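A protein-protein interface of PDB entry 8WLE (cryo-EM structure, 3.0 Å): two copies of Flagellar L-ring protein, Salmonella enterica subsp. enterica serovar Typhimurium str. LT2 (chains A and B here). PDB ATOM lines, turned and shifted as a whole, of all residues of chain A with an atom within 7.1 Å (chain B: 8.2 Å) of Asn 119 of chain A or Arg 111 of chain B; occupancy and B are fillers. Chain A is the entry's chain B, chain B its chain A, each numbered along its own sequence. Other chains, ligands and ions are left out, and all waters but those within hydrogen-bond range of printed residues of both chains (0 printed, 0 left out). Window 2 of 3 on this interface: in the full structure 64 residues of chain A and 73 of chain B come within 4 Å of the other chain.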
ATOM      1  N   PHE A 106     -21.164   2.251   0.148  1.00  0.00           N
ATOM      2  CA  PHE A 106     -21.628   0.870   0.263  1.00  0.00           C
ATOM      3  C   PHE A 106     -22.234   0.460  -1.077  1.00  0.00           C
ATOM      4  O   PHE A 106     -23.448   0.497  -1.292  1.00  0.00           O
ATOM      5  CB  PHE A 106     -22.620   0.730   1.407  1.00  0.00           C
ATOM      6  CG  PHE A 106     -22.288  -0.372   2.361  1.00  0.00           C
ATOM      7  CD1 PHE A 106     -21.884  -1.609   1.897  1.00  0.00           C
ATOM      8  CD2 PHE A 106     -22.368  -0.169   3.721  1.00  0.00           C
ATOM      9  CE1 PHE A 106     -21.577  -2.625   2.777  1.00  0.00           C
ATOM     10  CE2 PHE A 106     -22.064  -1.176   4.605  1.00  0.00           C
ATOM     11  CZ  PHE A 106     -21.668  -2.407   4.134  1.00  0.00           C
ATOM     12  N   VAL A 109     -24.967  -3.370  -0.545  1.00  0.00           N
ATOM     13  CA  VAL A 109     -25.293  -3.434   0.877  1.00  0.00           C
ATOM     14  C   VAL A 109     -25.839  -4.816   1.209  1.00  0.00           C
ATOM     15  O   VAL A 109     -26.790  -5.281   0.561  1.00  0.00           O
ATOM     16  CB  VAL A 109     -26.293  -2.337   1.276  1.00  0.00           C
ATOM     17  CG1 VAL A 109     -26.410  -2.259   2.785  1.00  0.00           C
ATOM     18  CG2 VAL A 109     -25.870  -1.001   0.710  1.00  0.00           C
ATOM     19  N   GLN A 114     -29.083  -3.226   5.437  1.00  0.00           N
ATOM     20  CA  GLN A 114     -29.766  -2.299   4.540  1.00  0.00           C
ATOM     21  C   GLN A 114     -30.633  -1.283   5.260  1.00  0.00           C
ATOM     22  O   GLN A 114     -31.140  -0.367   4.605  1.00  0.00           O
ATOM     23  CB  GLN A 114     -30.627  -3.060   3.534  1.00  0.00           C
ATOM     24  CG  GLN A 114     -29.853  -3.725   2.423  1.00  0.00           C
ATOM     25  CD  GLN A 114     -30.586  -3.660   1.101  1.00  0.00           C
ATOM     26  OE1 GLN A 114     -31.186  -2.642   0.764  1.00  0.00           O
ATOM     27  NE2 GLN A 114     -30.539  -4.750   0.346  1.00  0.00           N
ATOM     28  N   PHE A 117     -27.496   1.249   6.194  1.00  0.00           N
ATOM     29  CA  PHE A 117     -26.651   1.725   5.111  1.00  0.00           C
ATOM     30  C   PHE A 117     -27.293   1.613   3.738  1.00  0.00           C
ATOM     31  O   PHE A 117     -26.668   2.022   2.754  1.00  0.00           O
ATOM     32  CB  PHE A 117     -25.317   0.962   5.102  1.00  0.00           C
ATOM     33  CG  PHE A 117     -24.495   1.166   6.337  1.00  0.00           C
ATOM     34  CD1 PHE A 117     -23.726   2.302   6.488  1.00  0.00           C
ATOM     35  CD2 PHE A 117     -24.484   0.221   7.342  1.00  0.00           C
ATOM     36  CE1 PHE A 117     -22.969   2.494   7.618  1.00  0.00           C
ATOM     37  CE2 PHE A 117     -23.727   0.406   8.474  1.00  0.00           C
ATOM     38  CZ  PHE A 117     -22.968   1.545   8.613  1.00  0.00           C
ATOM     39  N   GLY A 118     -28.502   1.076   3.634  1.00  0.00           N
ATOM     40  CA  GLY A 118     -29.143   0.960   2.345  1.00  0.00           C
ATOM     41  C   GLY A 118     -29.635   2.295   1.825  1.00  0.00           C
ATOM     42  O   GLY A 118     -29.820   3.261   2.568  1.00  0.00           O
ATOM     43  N   ASN A 119     -29.842   2.343   0.509  1.00  0.00           N
ATOM     44  CA  ASN A 119     -30.353   3.533  -0.172  1.00  0.00           C
ATOM     45  C   ASN A 119     -29.453   4.745   0.073  1.00  0.00           C
ATOM     46  O   ASN A 119     -29.923   5.875   0.218  1.00  0.00           O
ATOM     47  CB  ASN A 119     -31.800   3.816   0.245  1.00  0.00           C
ATOM     48  CG  ASN A 119     -32.461   4.876  -0.609  1.00  0.00           C
ATOM     49  OD1 ASN A 119     -32.821   5.945  -0.119  1.00  0.00           O
ATOM     50  ND2 ASN A 119     -32.623   4.587  -1.894  1.00  0.00           N
ATOM     51  N   SER A 120     -28.143   4.501   0.121  1.00  0.00           N
ATOM     52  CA  SER A 120     -27.139   5.559   0.235  1.00  0.00           C
ATOM     53  C   SER A 120     -27.389   6.450   1.451  1.00  0.00           C
ATOM     54  O   SER A 120     -27.178   7.663   1.416  1.00  0.00           O
ATOM     55  CB  SER A 120     -27.082   6.393  -1.045  1.00  0.00           C
ATOM     56  OG  SER A 120     -26.859   5.574  -2.176  1.00  0.00           O
ATOM     57  N   ARG A 121     -27.847   5.839   2.544  1.00  0.00           N
ATOM     58  CA  ARG A 121     -28.119   6.595   3.761  1.00  0.00           C
ATOM     59  C   ARG A 121     -26.849   7.052   4.457  1.00  0.00           C
ATOM     60  O   ARG A 121     -26.891   8.022   5.222  1.00  0.00           O
ATOM     61  CB  ARG A 121     -28.962   5.761   4.723  1.00  0.00           C
ATOM     62  CG  ARG A 121     -30.448   5.986   4.582  1.00  0.00           C
ATOM     63  CD  ARG A 121     -31.235   5.105   5.527  1.00  0.00           C
ATOM     64  NE  ARG A 121     -31.391   3.754   5.008  1.00  0.00           N
ATOM     65  CZ  ARG A 121     -32.388   3.364   4.224  1.00  0.00           C
ATOM     66  NH1 ARG A 121     -33.324   4.209   3.822  1.00  0.00           N
ATOM     67  NH2 ARG A 121     -32.447   2.095   3.835  1.00  0.00           N
ATOM     68  N   ALA A 122     -25.729   6.385   4.212  1.00  0.00           N
ATOM     69  CA  ALA A 122     -24.444   6.784   4.763  1.00  0.00           C
ATOM     70  C   ALA A 122     -23.402   7.086   3.702  1.00  0.00           C
ATOM     71  O   ALA A 122     -22.402   7.740   4.010  1.00  0.00           O
ATOM     72  CB  ALA A 122     -23.898   5.702   5.703  1.00  0.00           C
ATOM     73  N   ASP A 123     -23.599   6.612   2.471  1.00  0.00           N
ATOM     74  CA  ASP A 123     -22.721   6.907   1.344  1.00  0.00           C
ATOM     75  C   ASP A 123     -22.462   8.404   1.236  1.00  0.00           C
ATOM     76  O   ASP A 123     -23.388   9.179   0.977  1.00  0.00           O
ATOM     77  CB  ASP A 123     -23.358   6.371   0.057  1.00  0.00           C
ATOM     78  CG  ASP A 123     -22.410   6.355  -1.121  1.00  0.00           C
ATOM     79  OD1 ASP A 123     -21.579   7.278  -1.253  1.00  0.00           O
ATOM     80  OD2 ASP A 123     -22.498   5.408  -1.931  1.00  0.00           O
ATOM     81  N   MET A 124     -21.212   8.817   1.428  1.00  0.00           N
ATOM     82  CA  MET A 124     -20.844  10.223   1.436  1.00  0.00           C
ATOM     83  C   MET A 124     -19.558  10.458   0.654  1.00  0.00           C
ATOM     84  O   MET A 124     -18.754   9.548   0.443  1.00  0.00           O
ATOM     85  CB  MET A 124     -20.664  10.743   2.861  1.00  0.00           C
ATOM     86  CG  MET A 124     -19.591  10.016   3.631  1.00  0.00           C
ATOM     87  SD  MET A 124     -18.766  11.111   4.796  1.00  0.00           S
ATOM     88  CE  MET A 124     -18.046  12.284   3.658  1.00  0.00           C
ATOM     89  N   PHE B 106     -19.420  19.302  -0.346  1.00  0.00           N
ATOM     90  CA  PHE B 106     -20.019  18.035   0.068  1.00  0.00           C
ATOM     91  C   PHE B 106     -20.704  17.415  -1.147  1.00  0.00           C
ATOM     92  O   PHE B 106     -21.913  17.534  -1.356  1.00  0.00           O
ATOM     93  CB  PHE B 106     -20.985  18.250   1.222  1.00  0.00           C
ATOM     94  CG  PHE B 106     -20.738  17.348   2.389  1.00  0.00           C
ATOM     95  CD1 PHE B 106     -20.477  16.004   2.200  1.00  0.00           C
ATOM     96  CD2 PHE B 106     -20.756  17.843   3.675  1.00  0.00           C
ATOM     97  CE1 PHE B 106     -20.248  15.173   3.276  1.00  0.00           C
ATOM     98  CE2 PHE B 106     -20.529  17.021   4.752  1.00  0.00           C
ATOM     99  CZ  PHE B 106     -20.276  15.684   4.554  1.00  0.00           C
ATOM    100  N   THR B 108     -21.367  14.357  -1.995  1.00  0.00           N
ATOM    101  CA  THR B 108     -22.395  13.386  -1.635  1.00  0.00           C
ATOM    102  C   THR B 108     -22.646  13.542  -0.144  1.00  0.00           C
ATOM    103  O   THR B 108     -21.803  13.159   0.671  1.00  0.00           O
ATOM    104  CB  THR B 108     -21.960  11.961  -1.972  1.00  0.00           C
ATOM    105  OG1 THR B 108     -21.619  11.878  -3.358  1.00  0.00           O
ATOM    106  CG2 THR B 108     -23.082  10.979  -1.672  1.00  0.00           C
ATOM    107  N   VAL B 109     -23.796  14.100   0.219  1.00  0.00           N
ATOM    108  CA  VAL B 109     -24.084  14.375   1.624  1.00  0.00           C
ATOM    109  C   VAL B 109     -24.758  13.162   2.250  1.00  0.00           C
ATOM    110  O   VAL B 109     -25.770  12.674   1.725  1.00  0.00           O
ATOM    111  CB  VAL B 109     -24.953  15.633   1.783  1.00  0.00           C
ATOM    112  CG1 VAL B 109     -25.016  16.043   3.242  1.00  0.00           C
ATOM    113  CG2 VAL B 109     -24.414  16.764   0.940  1.00  0.00           C
ATOM    114  N   PRO B 110     -24.240  12.647   3.362  1.00  0.00           N
ATOM    115  CA  PRO B 110     -24.940  11.571   4.066  1.00  0.00           C
ATOM    116  C   PRO B 110     -26.235  12.072   4.679  1.00  0.00           C
ATOM    117  O   PRO B 110     -26.385  13.255   4.995  1.00  0.00           O
ATOM    118  CB  PRO B 110     -23.939  11.143   5.143  1.00  0.00           C
ATOM    119  CG  PRO B 110     -23.056  12.319   5.325  1.00  0.00           C
ATOM    120  CD  PRO B 110     -22.944  12.969   3.984  1.00  0.00           C
ATOM    121  N   ARG B 111     -27.175  11.141   4.852  1.00  0.00           N
ATOM    122  CA  ARG B 111     -28.537  11.523   5.210  1.00  0.00           C
ATOM    123  C   ARG B 111     -28.621  12.148   6.596  1.00  0.00           C
ATOM    124  O   ARG B 111     -29.463  13.021   6.829  1.00  0.00           O
ATOM    125  CB  ARG B 111     -29.452  10.310   5.115  1.00  0.00           C
ATOM    126  CG  ARG B 111     -30.908  10.661   4.959  1.00  0.00           C
ATOM    127  CD  ARG B 111     -31.679   9.478   4.427  1.00  0.00           C
ATOM    128  NE  ARG B 111     -33.073   9.806   4.168  1.00  0.00           N
ATOM    129  CZ  ARG B 111     -33.948   8.962   3.641  1.00  0.00           C
ATOM    130  NH1 ARG B 111     -33.600   7.735   3.294  1.00  0.00           N
ATOM    131  NH2 ARG B 111     -35.204   9.358   3.462  1.00  0.00           N
ATOM    132  N   TYR B 112     -27.777  11.713   7.531  1.00  0.00           N
ATOM    133  CA  TYR B 112     -27.796  12.305   8.863  1.00  0.00           C
ATOM    134  C   TYR B 112     -27.214  13.710   8.887  1.00  0.00           C
ATOM    135  O   TYR B 112     -27.349  14.399   9.904  1.00  0.00           O
ATOM    136  CB  TYR B 112     -27.044  11.414   9.855  1.00  0.00           C
ATOM    137  CG  TYR B 112     -25.665  10.985   9.411  1.00  0.00           C
ATOM    138  CD1 TYR B 112     -25.479   9.805   8.711  1.00  0.00           C
ATOM    139  CD2 TYR B 112     -24.549  11.753   9.703  1.00  0.00           C
ATOM    140  CE1 TYR B 112     -24.222   9.403   8.307  1.00  0.00           C
ATOM    141  CE2 TYR B 112     -23.287  11.363   9.302  1.00  0.00           C
ATOM    142  CZ  TYR B 112     -23.131  10.186   8.605  1.00  0.00           C
ATOM    143  OH  TYR B 112     -21.881   9.787   8.203  1.00  0.00           O
ATOM    144  N   LEU B 113     -26.590  14.154   7.797  1.00  0.00           N
ATOM    145  CA  LEU B 113     -25.960  15.466   7.727  1.00  0.00           C
ATOM    146  C   LEU B 113     -26.569  16.357   6.655  1.00  0.00           C
ATOM    147  O   LEU B 113     -26.012  17.421   6.364  1.00  0.00           O
ATOM    148  CB  LEU B 113     -24.456  15.310   7.482  1.00  0.00           C
ATOM    149  CG  LEU B 113     -23.515  15.618   8.645  1.00  0.00           C
ATOM    150  CD1 LEU B 113     -24.151  15.257   9.971  1.00  0.00           C
ATOM    151  CD2 LEU B 113     -22.219  14.863   8.457  1.00  0.00           C
ATOM    152  N   GLN B 114     -27.692  15.954   6.060  1.00  0.00           N
ATOM    153  CA  GLN B 114     -28.304  16.736   4.989  1.00  0.00           C
ATOM    154  C   GLN B 114     -29.041  17.968   5.480  1.00  0.00           C
ATOM    155  O   GLN B 114     -29.471  18.772   4.647  1.00  0.00           O
ATOM    156  CB  GLN B 114     -29.268  15.873   4.178  1.00  0.00           C
ATOM    157  CG  GLN B 114     -28.601  14.908   3.231  1.00  0.00           C
ATOM    158  CD  GLN B 114     -29.362  14.766   1.932  1.00  0.00           C
ATOM    159  OE1 GLN B 114     -29.865  15.747   1.387  1.00  0.00           O
ATOM    160  NE2 GLN B 114     -29.450  13.541   1.428  1.00  0.00           N
ATOM    161  N   GLY B 115     -29.202  18.142   6.783  1.00  0.00           N
ATOM    162  CA  GLY B 115     -29.842  19.334   7.286  1.00  0.00           C
ATOM    163  C   GLY B 115     -28.825  20.421   7.546  1.00  0.00           C
ATOM    164  O   GLY B 115     -29.143  21.613   7.529  1.00  0.00           O
ATOM    165  N   LEU B 116     -27.582  20.007   7.786  1.00  0.00           N
ATOM    166  CA  LEU B 116     -26.495  20.941   8.020  1.00  0.00           C
ATOM    167  C   LEU B 116     -25.676  21.225   6.771  1.00  0.00           C
ATOM    168  O   LEU B 116     -25.089  22.305   6.667  1.00  0.00           O
ATOM    169  CB  LEU B 116     -25.572  20.400   9.112  1.00  0.00           C
ATOM    170  CG  LEU B 116     -25.105  21.393  10.171  1.00  0.00           C
ATOM    171  CD1 LEU B 116     -26.293  21.909  10.953  1.00  0.00           C
ATOM    172  CD2 LEU B 116     -24.100  20.738  11.093  1.00  0.00           C
ATOM    173  N   GLY B 118     -26.730  19.686   3.367  1.00  0.00           N
ATOM    174  CA  GLY B 118     -27.419  19.365   2.139  1.00  0.00           C
ATOM    175  C   GLY B 118     -27.787  20.603   1.347  1.00  0.00           C
ATOM    176  O   GLY B 118     -27.850  21.720   1.865  1.00  0.00           O
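N of Arg 111 of chain B lies within hydrogen-bond range of O of Arg 121 of chain A (3.2 Å).
The backbone carbonyl oxygen of Gln 114 of chain A sits at hydrogen-bond distance from the guanidinium group of Arg 121 of chain A (2.9 Å). The guanidinium group (NE) of Arg 121 of chain A lies within hydrogen-bond range of the backbone carbonyl oxygen (O) of Gly 118 of chain A (2.9 Å).
Arg 111 of chain B touches Asn 119 of chain A. Pro 110 of chain B touches Ala 122 of chain A. Asp 123 of chain A touches Thr 108 of chain B (O to CG2, 3.2 Å). CE1 of Phe 106 of chain B touches CE of Met 124 of chain A (3.7 Å). Met 124 of chain A touches Thr 108 of chain B (CA to O, 3.2 Å). Pro 110 of chain B touches Met 124 of chain A.
Of chain B, only Arg 111 comes within 4 Å of Asn 119 of chain A. Of chain A, only Asn 119 (3.9 Å) and Arg 121 (3.2 Å) come within 4 Å of Arg 111 of chain B. No residue of chain B comes within 4 Å of Gly 118 of chain A. No residue of chain B comes within 4 Å of Ser 120 of chain A. Of the printed residues of chain A, Phe 106 of chain B touches Met 124. Of the printed residues of chain A, Pro 110 of chain B touches Ala 122 (3.9 Å) and Met 124 (3.4 Å). Val 109 of chain B touches none of the printed residues of chain A. Gly 118 of chain B touches none of the printed residues of chain A. The nearest residue of chain B that does not touch Asn 119 of chain A is Gln 114 of chain B (7.8 Å).
Of the 11 printed residues of chain A, 5 touch a printed residue of chain B. Hydrophobic or aromatic side chains of chain A that line the printed part of chain B: Met 124. Of the 11 printed residues of chain B, 4 touch a printed residue of chain A. Among the printed residues, 7 pairs touch across the chains.
Positions printed for both chains: 106, 109, 114 and 118.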
